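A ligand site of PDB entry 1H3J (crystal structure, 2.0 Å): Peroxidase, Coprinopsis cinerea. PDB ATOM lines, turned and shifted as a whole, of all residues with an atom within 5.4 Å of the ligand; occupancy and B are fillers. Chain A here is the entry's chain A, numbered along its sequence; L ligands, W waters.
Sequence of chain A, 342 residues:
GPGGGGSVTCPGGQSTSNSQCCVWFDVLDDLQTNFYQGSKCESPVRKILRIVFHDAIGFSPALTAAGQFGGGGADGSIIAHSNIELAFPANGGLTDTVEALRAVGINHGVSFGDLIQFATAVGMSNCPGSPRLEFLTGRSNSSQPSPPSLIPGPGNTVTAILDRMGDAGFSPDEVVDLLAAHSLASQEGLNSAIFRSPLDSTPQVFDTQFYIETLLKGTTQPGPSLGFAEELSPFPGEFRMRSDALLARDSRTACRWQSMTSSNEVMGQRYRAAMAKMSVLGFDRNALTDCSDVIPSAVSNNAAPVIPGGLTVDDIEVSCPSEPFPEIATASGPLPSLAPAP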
ATOM      1  N   SER A  43      35.239   4.713  -6.375  1.00  0.00           N
ATOM      2  CA  SER A  43      34.761   5.638  -5.352  1.00  0.00           C
ATOM      3  C   SER A  43      33.431   6.360  -5.639  1.00  0.00           C
ATOM      4  O   SER A  43      32.531   6.345  -4.799  1.00  0.00           O
ATOM      5  CB  SER A  43      35.840   6.624  -4.974  1.00  0.00           C
ATOM      6  OG  SER A  43      35.471   7.298  -3.785  1.00  0.00           O
ATOM      7  N   VAL A  45      30.698   5.572  -7.136  1.00  0.00           N
ATOM      8  CA  VAL A  45      29.507   4.758  -6.803  1.00  0.00           C
ATOM      9  C   VAL A  45      29.320   4.639  -5.288  1.00  0.00           C
ATOM     10  O   VAL A  45      28.206   4.641  -4.794  1.00  0.00           O
ATOM     11  CB  VAL A  45      29.594   3.304  -7.346  1.00  0.00           C
ATOM     12  CG1 VAL A  45      28.349   2.548  -6.949  1.00  0.00           C
ATOM     13  CG2 VAL A  45      29.739   3.284  -8.859  1.00  0.00           C
ATOM     14  N   ARG A  46      30.433   4.485  -4.574  1.00  0.00           N
ATOM     15  CA  ARG A  46      30.415   4.325  -3.124  1.00  0.00           C
ATOM     16  C   ARG A  46      29.924   5.603  -2.435  1.00  0.00           C
ATOM     17  O   ARG A  46      29.098   5.547  -1.515  1.00  0.00           O
ATOM     18  CB  ARG A  46      31.793   3.891  -2.648  1.00  0.00           C
ATOM     19  CG  ARG A  46      32.252   2.586  -3.307  1.00  0.00           C
ATOM     20  CD  ARG A  46      33.394   1.905  -2.547  1.00  0.00           C
ATOM     21  NE  ARG A  46      34.523   2.804  -2.294  1.00  0.00           N
ATOM     22  CZ  ARG A  46      35.622   2.872  -3.033  1.00  0.00           C
ATOM     23  NH1 ARG A  46      35.779   2.086  -4.097  1.00  0.00           N
ATOM     24  NH2 ARG A  46      36.575   3.723  -2.714  1.00  0.00           N
ATOM     25  N   LYS A  47      30.406   6.747  -2.905  1.00  0.00           N
ATOM     26  CA  LYS A  47      30.018   8.054  -2.413  1.00  0.00           C
ATOM     27  C   LYS A  47      28.522   8.289  -2.687  1.00  0.00           C
ATOM     28  O   LYS A  47      27.793   8.781  -1.809  1.00  0.00           O
ATOM     29  CB  LYS A  47      30.818   9.137  -3.103  1.00  0.00           C
ATOM     30  CG  LYS A  47      32.321   9.114  -2.834  1.00  0.00           C
ATOM     31  CD  LYS A  47      32.609   9.435  -1.393  1.00  0.00           C
ATOM     32  CE  LYS A  47      34.087   9.700  -1.167  1.00  0.00           C
ATOM     33  NZ  LYS A  47      34.260  10.027   0.271  1.00  0.00           N
ATOM     34  N   LEU A  49      26.184   6.091  -3.011  1.00  0.00           N
ATOM     35  CA  LEU A  49      25.386   5.212  -2.155  1.00  0.00           C
ATOM     36  C   LEU A  49      25.244   5.811  -0.743  1.00  0.00           C
ATOM     37  O   LEU A  49      24.191   5.639  -0.103  1.00  0.00           O
ATOM     38  CB  LEU A  49      25.982   3.793  -2.099  1.00  0.00           C
ATOM     39  CG  LEU A  49      25.564   2.804  -3.179  1.00  0.00           C
ATOM     40  CD1 LEU A  49      26.405   1.562  -3.081  1.00  0.00           C
ATOM     41  CD2 LEU A  49      24.137   2.450  -3.019  1.00  0.00           C
ATOM     42  N   ARG A  50      26.287   6.501  -0.281  1.00  0.00           N
ATOM     43  CA  ARG A  50      26.247   7.197   1.016  1.00  0.00           C
ATOM     44  C   ARG A  50      25.224   8.334   0.849  1.00  0.00           C
ATOM     45  O   ARG A  50      24.365   8.565   1.708  1.00  0.00           O
ATOM     46  CB  ARG A  50      27.610   7.830   1.333  1.00  0.00           C
ATOM     47  CG  ARG A  50      28.500   7.037   2.258  1.00  0.00           C
ATOM     48  CD  ARG A  50      29.753   7.844   2.664  1.00  0.00           C
ATOM     49  NE  ARG A  50      29.525   8.818   3.740  1.00  0.00           N
ATOM     50  CZ  ARG A  50      30.300   9.872   3.977  1.00  0.00           C
ATOM     51  NH1 ARG A  50      31.356  10.098   3.228  1.00  0.00           N
ATOM     52  NH2 ARG A  50      30.024  10.713   4.957  1.00  0.00           N
ATOM     53  N   VAL A  52      22.631   8.706  -1.336  1.00  0.00           N
ATOM     54  CA  VAL A  52      21.228   8.348  -1.387  1.00  0.00           C
ATOM     55  C   VAL A  52      20.627   8.075  -0.004  1.00  0.00           C
ATOM     56  O   VAL A  52      19.517   8.542   0.313  1.00  0.00           O
ATOM     57  CB  VAL A  52      20.956   7.165  -2.392  1.00  0.00           C
ATOM     58  CG1 VAL A  52      21.581   5.852  -1.928  1.00  0.00           C
ATOM     59  CG2 VAL A  52      19.459   7.012  -2.623  1.00  0.00           C
ATOM     60  N   PHE A  53      21.337   7.311   0.836  1.00  0.00           N
ATOM     61  CA  PHE A  53      20.887   7.006   2.196  1.00  0.00           C
ATOM     62  C   PHE A  53      20.774   8.289   3.050  1.00  0.00           C
ATOM     63  O   PHE A  53      19.768   8.508   3.713  1.00  0.00           O
ATOM     64  CB  PHE A  53      21.884   6.011   2.838  1.00  0.00           C
ATOM     65  CG  PHE A  53      21.627   5.715   4.294  1.00  0.00           C
ATOM     66  CD1 PHE A  53      22.685   5.694   5.209  1.00  0.00           C
ATOM     67  CD2 PHE A  53      20.329   5.465   4.770  1.00  0.00           C
ATOM     68  CE1 PHE A  53      22.447   5.414   6.576  1.00  0.00           C
ATOM     69  CE2 PHE A  53      20.084   5.195   6.107  1.00  0.00           C
ATOM     70  CZ  PHE A  53      21.132   5.170   7.026  1.00  0.00           C
ATOM     71  N   PRO A 152      21.766   7.846  11.250  1.00  0.00           N
ATOM     72  CA  PRO A 152      22.423   6.959  12.229  1.00  0.00           C
ATOM     73  C   PRO A 152      23.954   7.059  12.105  1.00  0.00           C
ATOM     74  O   PRO A 152      24.487   7.181  10.993  1.00  0.00           O
ATOM     75  CB  PRO A 152      21.950   5.569  11.821  1.00  0.00           C
ATOM     76  CG  PRO A 152      20.603   5.800  11.198  1.00  0.00           C
ATOM     77  CD  PRO A 152      20.788   7.097  10.419  1.00  0.00           C
ATOM     78  N   GLY A 153      24.651   7.027  13.236  1.00  0.00           N
ATOM     79  CA  GLY A 153      26.105   7.109  13.205  1.00  0.00           C
ATOM     80  C   GLY A 153      26.750   5.788  13.605  1.00  0.00           C
ATOM     81  O   GLY A 153      26.129   4.968  14.293  1.00  0.00           O
ATOM     82  N   PRO A 154      28.027   5.581  13.258  1.00  0.00           N
ATOM     83  CA  PRO A 154      28.733   4.337  13.587  1.00  0.00           C
ATOM     84  C   PRO A 154      28.988   4.105  15.072  1.00  0.00           C
ATOM     85  O   PRO A 154      29.342   3.001  15.441  1.00  0.00           O
ATOM     86  CB  PRO A 154      30.028   4.461  12.804  1.00  0.00           C
ATOM     87  CG  PRO A 154      30.288   5.955  12.857  1.00  0.00           C
ATOM     88  CD  PRO A 154      28.903   6.533  12.568  1.00  0.00           C
ATOM     89  N   ILE A 161      19.898   2.896  16.565  1.00  0.00           N
ATOM     90  CA  ILE A 161      19.813   2.728  15.112  1.00  0.00           C
ATOM     91  C   ILE A 161      18.431   2.225  14.712  1.00  0.00           C
ATOM     92  O   ILE A 161      17.782   2.791  13.831  1.00  0.00           O
ATOM     93  CB  ILE A 161      20.925   1.744  14.608  1.00  0.00           C
ATOM     94  CG1 ILE A 161      22.302   2.372  14.808  1.00  0.00           C
ATOM     95  CG2 ILE A 161      20.735   1.423  13.144  1.00  0.00           C
ATOM     96  CD1 ILE A 161      23.478   1.436  14.680  1.00  0.00           C
ATOM     97  N   MET A 165      15.730   4.309  12.406  1.00  0.00           N
ATOM     98  CA  MET A 165      15.302   3.658  11.170  1.00  0.00           C
ATOM     99  C   MET A 165      13.840   3.241  11.254  1.00  0.00           C
ATOM    100  O   MET A 165      13.094   3.369  10.280  1.00  0.00           O
ATOM    101  CB  MET A 165      16.186   2.449  10.867  1.00  0.00           C
ATOM    102  CG  MET A 165      17.685   2.785  10.641  1.00  0.00           C
ATOM    103  SD  MET A 165      17.972   3.728   9.175  1.00  0.00           S
ATOM    104  CE  MET A 165      17.923   2.430   7.955  1.00  0.00           C
ATOM    105  N   VAL A 175      16.563  -3.002   7.958  1.00  0.00           N
ATOM    106  CA  VAL A 175      17.805  -2.327   8.316  1.00  0.00           C
ATOM    107  C   VAL A 175      18.997  -3.208   7.896  1.00  0.00           C
ATOM    108  O   VAL A 175      19.961  -2.717   7.284  1.00  0.00           O
ATOM    109  CB  VAL A 175      17.848  -1.995   9.815  1.00  0.00           C
ATOM    110  CG1 VAL A 175      19.223  -1.460  10.183  1.00  0.00           C
ATOM    111  CG2 VAL A 175      16.750  -0.978  10.142  1.00  0.00           C
ATOM    112  N   LEU A 178      19.213  -3.254   3.984  1.00  0.00           N
ATOM    113  CA  LEU A 178      19.741  -1.996   3.447  1.00  0.00           C
ATOM    114  C   LEU A 178      21.268  -1.934   3.607  1.00  0.00           C
ATOM    115  O   LEU A 178      21.969  -1.329   2.784  1.00  0.00           O
ATOM    116  CB  LEU A 178      19.094  -0.835   4.200  1.00  0.00           C
ATOM    117  CG  LEU A 178      18.196   0.213   3.561  1.00  0.00           C
ATOM    118  CD1 LEU A 178      17.766  -0.129   2.158  1.00  0.00           C
ATOM    119  CD2 LEU A 178      17.039   0.441   4.484  1.00  0.00           C
ATOM    120  N   LEU A 179      21.771  -2.576   4.654  1.00  0.00           N
ATOM    121  CA  LEU A 179      23.217  -2.601   4.906  1.00  0.00           C
ATOM    122  C   LEU A 179      24.024  -3.420   3.905  1.00  0.00           C
ATOM    123  O   LEU A 179      25.246  -3.425   3.961  1.00  0.00           O
ATOM    124  CB  LEU A 179      23.522  -3.026   6.356  1.00  0.00           C
ATOM    125  CG  LEU A 179      23.593  -1.803   7.296  1.00  0.00           C
ATOM    126  CD1 LEU A 179      23.359  -2.206   8.720  1.00  0.00           C
ATOM    127  CD2 LEU A 179      24.895  -1.063   7.107  1.00  0.00           C
ATOM    128  N   ALA A 181      24.626  -2.555   1.175  1.00  0.00           N
ATOM    129  CA  ALA A 181      25.429  -1.548   0.492  1.00  0.00           C
ATOM    130  C   ALA A 181      26.880  -1.494   0.989  1.00  0.00           C
ATOM    131  O   ALA A 181      27.769  -1.017   0.291  1.00  0.00           O
ATOM    132  CB  ALA A 181      24.774  -0.148   0.610  1.00  0.00           C
ATOM    133  N   HIS A 182      27.127  -1.968   2.215  1.00  0.00           N
ATOM    134  CA  HIS A 182      28.493  -1.988   2.761  1.00  0.00           C
ATOM    135  C   HIS A 182      29.351  -3.078   2.100  1.00  0.00           C
ATOM    136  O   HIS A 182      30.522  -3.236   2.409  1.00  0.00           O
ATOM    137  CB  HIS A 182      28.488  -2.161   4.296  1.00  0.00           C
ATOM    138  CG  HIS A 182      28.235  -0.850   5.023  1.00  0.00           C
ATOM    139  ND1 HIS A 182      28.326  -0.725   6.379  1.00  0.00           N
ATOM    140  CD2 HIS A 182      27.905   0.390   4.472  1.00  0.00           C
ATOM    141  CE1 HIS A 182      28.035   0.547   6.628  1.00  0.00           C
ATOM    142  NE2 HIS A 182      27.753   1.253   5.569  1.00  0.00           N
ATOM    143  N   LEU A 184      29.956  -2.815  -0.841  1.00  0.00           N
ATOM    144  CA  LEU A 184      30.645  -1.981  -1.851  1.00  0.00           C
ATOM    145  C   LEU A 184      31.057  -0.739  -1.064  1.00  0.00           C
ATOM    146  O   LEU A 184      30.611   0.375  -1.368  1.00  0.00           O
ATOM    147  CB  LEU A 184      29.657  -1.543  -2.934  1.00  0.00           C
ATOM    148  CG  LEU A 184      29.069  -2.653  -3.842  1.00  0.00           C
ATOM    149  CD1 LEU A 184      27.883  -2.123  -4.587  1.00  0.00           C
ATOM    150  CD2 LEU A 184      30.138  -3.131  -4.829  1.00  0.00           C
ATOM    151  N   ALA A 185      31.938  -0.908  -0.082  1.00  0.00           N
ATOM    152  CA  ALA A 185      32.288   0.189   0.806  1.00  0.00           C
ATOM    153  C   ALA A 185      33.683   0.180   1.371  1.00  0.00           C
ATOM    154  O   ALA A 185      34.299  -0.882   1.555  1.00  0.00           O
ATOM    155  CB  ALA A 185      31.308   0.188   1.971  1.00  0.00           C
ATOM    156  N   SER A 186      34.124   1.371   1.772  1.00  0.00           N
ATOM    157  CA  SER A 186      35.408   1.604   2.394  1.00  0.00           C
ATOM    158  C   SER A 186      35.145   2.769   3.366  1.00  0.00           C
ATOM    159  O   SER A 186      34.006   3.196   3.501  1.00  0.00           O
ATOM    160  CB  SER A 186      36.449   2.005   1.333  1.00  0.00           C
ATOM    161  OG  SER A 186      36.369   3.370   0.950  1.00  0.00           O
ATOM    162  N   GLN A 187      36.157   3.213   4.104  1.00  0.00           N
ATOM    163  CA  GLN A 187      36.014   4.361   4.987  1.00  0.00           C
ATOM    164  C   GLN A 187      37.161   5.264   4.676  1.00  0.00           C
ATOM    165  O   GLN A 187      38.243   4.796   4.350  1.00  0.00           O
ATOM    166  CB  GLN A 187      35.961   3.973   6.491  1.00  0.00           C
ATOM    167  CG  GLN A 187      37.242   3.373   7.143  1.00  0.00           C
ATOM    168  CD  GLN A 187      38.375   4.377   7.338  1.00  0.00           C
ATOM    169  OE1 GLN A 187      38.132   5.561   7.575  1.00  0.00           O
ATOM    170  NE2 GLN A 187      39.606   3.929   7.150  1.00  0.00           N
ATOM    171  N   GLU A 188      36.927   6.562   4.662  1.00  0.00           N
ATOM    172  CA  GLU A 188      37.994   7.503   4.394  1.00  0.00           C
ATOM    173  C   GLU A 188      38.144   8.408   5.612  1.00  0.00           C
ATOM    174  O   GLU A 188      39.222   8.900   5.891  1.00  0.00           O
ATOM    175  CB  GLU A 188      37.655   8.372   3.189  1.00  0.00           C
ATOM    176  CG  GLU A 188      37.470   7.588   1.919  1.00  0.00           C
ATOM    177  CD  GLU A 188      37.271   8.484   0.722  1.00  0.00           C
ATOM    178  OE1 GLU A 188      36.989   9.681   0.876  1.00  0.00           O
ATOM    179  OE2 GLU A 188      37.402   7.965  -0.405  1.00  0.00           O
ATOM    180  N   GLY A 189      37.048   8.581   6.344  1.00  0.00           N
ATOM    181  CA  GLY A 189      37.086   9.443   7.497  1.00  0.00           C
ATOM    182  C   GLY A 189      37.167   8.839   8.895  1.00  0.00           C
ATOM    183  O   GLY A 189      37.374   9.597   9.834  1.00  0.00           O
ATOM    184  N   LEU A 190      36.950   7.539   9.078  1.00  0.00           N
ATOM    185  CA  LEU A 190      37.020   7.009  10.451  1.00  0.00           C
ATOM    186  C   LEU A 190      38.470   6.803  10.922  1.00  0.00           C
ATOM    187  O   LEU A 190      38.763   6.964  12.111  1.00  0.00           O
ATOM    188  CB  LEU A 190      36.211   5.721  10.591  1.00  0.00           C
ATOM    189  CG  LEU A 190      34.715   5.820  10.242  1.00  0.00           C
ATOM    190  CD1 LEU A 190      34.090   4.454  10.426  1.00  0.00           C
ATOM    191  CD2 LEU A 190      34.031   6.812  11.121  1.00  0.00           C
ATOM    192  N   LEU A 199      35.323  -2.518   3.624  1.00  0.00           N
ATOM    193  CA  LEU A 199      34.528  -3.127   4.660  1.00  0.00           C
ATOM    194  C   LEU A 199      34.386  -4.639   4.397  1.00  0.00           C
ATOM    195  O   LEU A 199      33.855  -5.369   5.243  1.00  0.00           O
ATOM    196  CB  LEU A 199      33.160  -2.425   4.772  1.00  0.00           C
ATOM    197  CG  LEU A 199      33.020  -1.170   5.686  1.00  0.00           C
ATOM    198  CD1 LEU A 199      34.262  -0.324   5.736  1.00  0.00           C
ATOM    199  CD2 LEU A 199      31.812  -0.344   5.307  1.00  0.00           C
ATOM    200  N   MET A 241      33.567  -1.495  11.292  1.00  0.00           N
ATOM    201  CA  MET A 241      33.013  -0.418  12.099  1.00  0.00           C
ATOM    202  C   MET A 241      32.105  -0.993  13.184  1.00  0.00           C
ATOM    203  O   MET A 241      31.478  -2.045  13.021  1.00  0.00           O
ATOM    204  CB  MET A 241      32.329   0.697  11.251  1.00  0.00           C
ATOM    205  CG  MET A 241      30.905   0.462  10.829  1.00  0.00           C
ATOM    206  SD  MET A 241      30.249   1.923   9.906  1.00  0.00           S
ATOM    207  CE  MET A 241      31.143   1.777   8.398  1.00  0.00           C
ATOM    208  N   SER A 243      29.140  -0.173  14.562  1.00  0.00           N
ATOM    209  CA  SER A 243      27.719  -0.401  14.315  1.00  0.00           C
ATOM    210  C   SER A 243      27.502  -1.726  13.566  1.00  0.00           C
ATOM    211  O   SER A 243      26.578  -2.468  13.888  1.00  0.00           O
ATOM    212  CB  SER A 243      27.102   0.762  13.497  1.00  0.00           C
ATOM    213  OG  SER A 243      27.949   1.103  12.412  1.00  0.00           O
ATOM    214  N   LEU A 247      25.397  -4.896  14.967  1.00  0.00           N
ATOM    215  CA  LEU A 247      24.181  -5.378  14.274  1.00  0.00           C
ATOM    216  C   LEU A 247      24.295  -6.845  13.885  1.00  0.00           C
ATOM    217  O   LEU A 247      23.301  -7.556  13.892  1.00  0.00           O
ATOM    218  CB  LEU A 247      23.846  -4.516  13.045  1.00  0.00           C
ATOM    219  CG  LEU A 247      23.330  -3.108  13.385  1.00  0.00           C
ATOM    220  CD1 LEU A 247      23.515  -2.180  12.203  1.00  0.00           C
ATOM    221  CD2 LEU A 247      21.863  -3.157  13.841  1.00  0.00           C
ATOM    222  N   TYR A 271      17.588  -6.383  -0.787  1.00  0.00           N
ATOM    223  CA  TYR A 271      18.165  -5.068  -0.875  1.00  0.00           C
ATOM    224  C   TYR A 271      17.381  -4.203  -1.859  1.00  0.00           C
ATOM    225  O   TYR A 271      17.113  -3.054  -1.584  1.00  0.00           O
ATOM    226  CB  TYR A 271      19.630  -5.187  -1.300  1.00  0.00           C
ATOM    227  CG  TYR A 271      20.287  -3.844  -1.562  1.00  0.00           C
ATOM    228  CD1 TYR A 271      20.620  -3.474  -2.875  1.00  0.00           C
ATOM    229  CD2 TYR A 271      20.632  -2.992  -0.532  1.00  0.00           C
ATOM    230  CE1 TYR A 271      21.270  -2.330  -3.145  1.00  0.00           C
ATOM    231  CE2 TYR A 271      21.298  -1.819  -0.792  1.00  0.00           C
ATOM    232  CZ  TYR A 271      21.611  -1.502  -2.099  1.00  0.00           C
ATOM    233  OH  TYR A 271      22.320  -0.383  -2.417  1.00  0.00           O
ATOM    234  N   MET A 275      15.539  -0.747  -0.878  1.00  0.00           N
ATOM    235  CA  MET A 275      15.896   0.475  -1.585  1.00  0.00           C
ATOM    236  C   MET A 275      14.640   1.122  -2.265  1.00  0.00           C
ATOM    237  O   MET A 275      14.491   2.356  -2.246  1.00  0.00           O
ATOM    238  CB  MET A 275      16.976   0.214  -2.635  1.00  0.00           C
ATOM    239  CG  MET A 275      18.337  -0.082  -2.067  1.00  0.00           C
ATOM    240  SD  MET A 275      19.069   1.318  -1.159  1.00  0.00           S
ATOM    241  CE  MET A 275      19.772   2.381  -2.447  1.00  0.00           C
ATOM    242  N   MET A 278      12.989   2.981   0.263  1.00  0.00           N
ATOM    243  CA  MET A 278      13.688   4.147   0.712  1.00  0.00           C
ATOM    244  C   MET A 278      13.665   5.225  -0.333  1.00  0.00           C
ATOM    245  O   MET A 278      13.726   6.412  -0.007  1.00  0.00           O
ATOM    246  CB  MET A 278      15.139   3.810   1.065  1.00  0.00           C
ATOM    247  CG  MET A 278      15.885   4.973   1.647  1.00  0.00           C
ATOM    248  SD  MET A 278      17.547   4.567   2.197  1.00  0.00           S
ATOM    249  CE  MET A 278      18.456   4.771   0.753  1.00  0.00           C
HETATM  250  C1  LIG L   1      30.498   4.000   4.393  1.00  0.00           C
HETATM  251  C2  LIG L   1      27.957   4.282   8.555  1.00  0.00           C
HETATM  252  C3  LIG L   1      23.964   2.383   6.479  1.00  0.00           C
HETATM  253  C4  LIG L   1      26.193   2.983   2.197  1.00  0.00           C
HETATM  254  C5  LIG L   1      30.097   4.425   5.646  1.00  0.00           C
HETATM  255  C6  LIG L   1      30.920   5.028   6.634  1.00  0.00           C
HETATM  256  C7  LIG L   1      30.162   5.157   7.779  1.00  0.00           C
HETATM  257  C8  LIG L   1      28.928   4.528   7.545  1.00  0.00           C
HETATM  258  C9  LIG L   1      30.567   5.837   9.068  1.00  0.00           C
HETATM  259  C10 LIG L   1      32.368   5.391   6.475  1.00  0.00           C
HETATM  260  C11 LIG L   1      32.424   6.629   5.607  1.00  0.00           C
HETATM  261  C12 LIG L   1      33.782   7.300   5.600  1.00  0.00           C
HETATM  262  O1  LIG L   1      34.355   7.503   6.685  1.00  0.00           O
HETATM  263  O2  LIG L   1      34.295   7.629   4.519  1.00  0.00           O
HETATM  264  C13 LIG L   1      26.692   3.688   8.387  1.00  0.00           C
HETATM  265  C14 LIG L   1      25.772   3.519   9.398  1.00  0.00           C
HETATM  266  C15 LIG L   1      24.695   2.891   8.812  1.00  0.00           C
HETATM  267  C16 LIG L   1      24.946   2.741   7.431  1.00  0.00           C
HETATM  268  C17 LIG L   1      25.841   3.872  10.894  1.00  0.00           C
HETATM  269  C18 LIG L   1      23.440   2.637   9.413  1.00  0.00           C
HETATM  270  C19 LIG L   1      22.912   1.510  10.068  1.00  0.00           C
HETATM  271  C20 LIG L   1      24.182   2.505   5.072  1.00  0.00           C
HETATM  272  C21 LIG L   1      23.170   2.406   4.017  1.00  0.00           C
HETATM  273  C22 LIG L   1      23.761   2.657   2.829  1.00  0.00           C
HETATM  274  C23 LIG L   1      25.182   2.835   3.149  1.00  0.00           C
HETATM  275  C24 LIG L   1      21.707   2.024   4.319  1.00  0.00           C
HETATM  276  C25 LIG L   1      23.257   2.792   1.484  1.00  0.00           C
HETATM  277  C26 LIG L   1      22.208   2.072   0.962  1.00  0.00           C
HETATM  278  C27 LIG L   1      27.556   3.221   2.415  1.00  0.00           C
HETATM  279  C28 LIG L   1      28.578   3.106   1.410  1.00  0.00           C
HETATM  280  C29 LIG L   1      29.749   3.456   2.017  1.00  0.00           C
HETATM  281  C30 LIG L   1      29.479   3.695   3.419  1.00  0.00           C
HETATM  282  C31 LIG L   1      28.474   2.536  -0.022  1.00  0.00           C
HETATM  283  C32 LIG L   1      31.127   3.495   1.360  1.00  0.00           C
HETATM  284  C33 LIG L   1      31.650   4.888   1.122  1.00  0.00           C
HETATM  285  C34 LIG L   1      33.019   4.887   0.507  1.00  0.00           C
HETATM  286  O3  LIG L   1      33.548   5.975   0.166  1.00  0.00           O
HETATM  287  O4  LIG L   1      33.604   3.798   0.353  1.00  0.00           O
HETATM  288  N1  LIG L   1      28.865   4.122   6.175  1.00  0.00           N
HETATM  289  N2  LIG L   1      26.170   3.259   7.149  1.00  0.00           N
HETATM  290  N3  LIG L   1      25.406   2.829   4.522  1.00  0.00           N
HETATM  291  N4  LIG L   1      28.105   3.552   3.663  1.00  0.00           N
HETATM  292 FE1  LIG L   1      27.206   3.370   5.399  1.00  0.00          FE
HETATM  293  O   HOH W   1      33.136   8.031   1.919  1.00  0.00           O
HETATM  294  O   HOH W   2      28.421   7.909   6.501  1.00  0.00           O
HETATM  295  O   HOH W   3      33.119   9.063   8.450  1.00  0.00           O
HETATM  296  O   HOH W   4      35.616   5.999  -1.405  1.00  0.00           O
HETATM  297  O   HOH W   5      26.332   5.648   5.522  1.00  0.00           O
HETATM  298  O   HOH W   6      34.454  10.559   4.145  1.00  0.00           O
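Water W4 lies within hydrogen-bond range of O3 of the ligand, OG of Ser 43, NH2 of Arg 46 and OE2 of Glu 188. Water W1 lies within hydrogen-bond range of O3 of the ligand, NZ of Lys 47 and NH1 of Arg 50. Water W6 bridges an oxygen (O2) of the ligand and the guanidinium group of Arg 50.
An oxygen (O4) of the ligand sits at hydrogen-bond distance from the side-chain hydroxyl (OG) of Ser 186 (2.9 Å). The guanidinium group (NE) of Arg 46 lies within salt-bridge range of an oxygen (O4) of the ligand (3.0 Å). O2 of the ligand lies within hydrogen-bond range of N of Glu 188 (2.8 Å). NE2 of His 182 is bound to FE1 of the ligand, at 2.2 Å. N of Ser 186 is in hydrogen-bond range of O4 of the ligand, 2.9 Å away. O1 of the ligand sits at hydrogen-bond distance from N of Gly 189 (2.9 Å).
The side-chain carboxylate of Glu 188 is in salt-bridge range of the side-chain amino group of Lys 47. The backbone carbonyl oxygen of Ala 185 is in hydrogen-bond range of the backbone NH of Leu 199 (2.8 Å). O of Pro 154 is in hydrogen-bond range of N of Ser 243 (3.3 Å). N of Leu 190 is in hydrogen-bond range of OE1 of Gln 187 (2.8 Å). N of Gly 189 is in hydrogen-bond range of OE1 of Gln 187 (3.4 Å). The side-chain hydroxyl of Ser 243 lies close to the side-chain sulfur of Met 241, at 3.5 Å.
Merely in contact with the ligand: Lys 47, Leu 49, Arg 50, Phe 53, Pro 152, Gly 153, Pro 154, Ile 161, Leu 178, Leu 179, Ala 181, Leu 184, Ala 185, Gln 187, Leu 190, Met 241, Ser 243 and Met 275. Hydrophobic or aromatic side chains within 4 Å of the ligand: Leu 49, Phe 53, Pro 154, Ile 161, Leu 178, Leu 179, Ala 181, His 182, Ala 185, Leu 190, Met 241 and Met 275. Within 4 Å of the ligand: Arg 46, Lys 47, Leu 49, Arg 50, Phe 53, Pro 152, Gly 153, Pro 154, Ile 161, Leu 178, Leu 179, Ala 181, His 182, Leu 184, Ala 185, Ser 186, Gln 187, Glu 188, Gly 189, Leu 190, Met 241, Ser 243 and Met 275.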
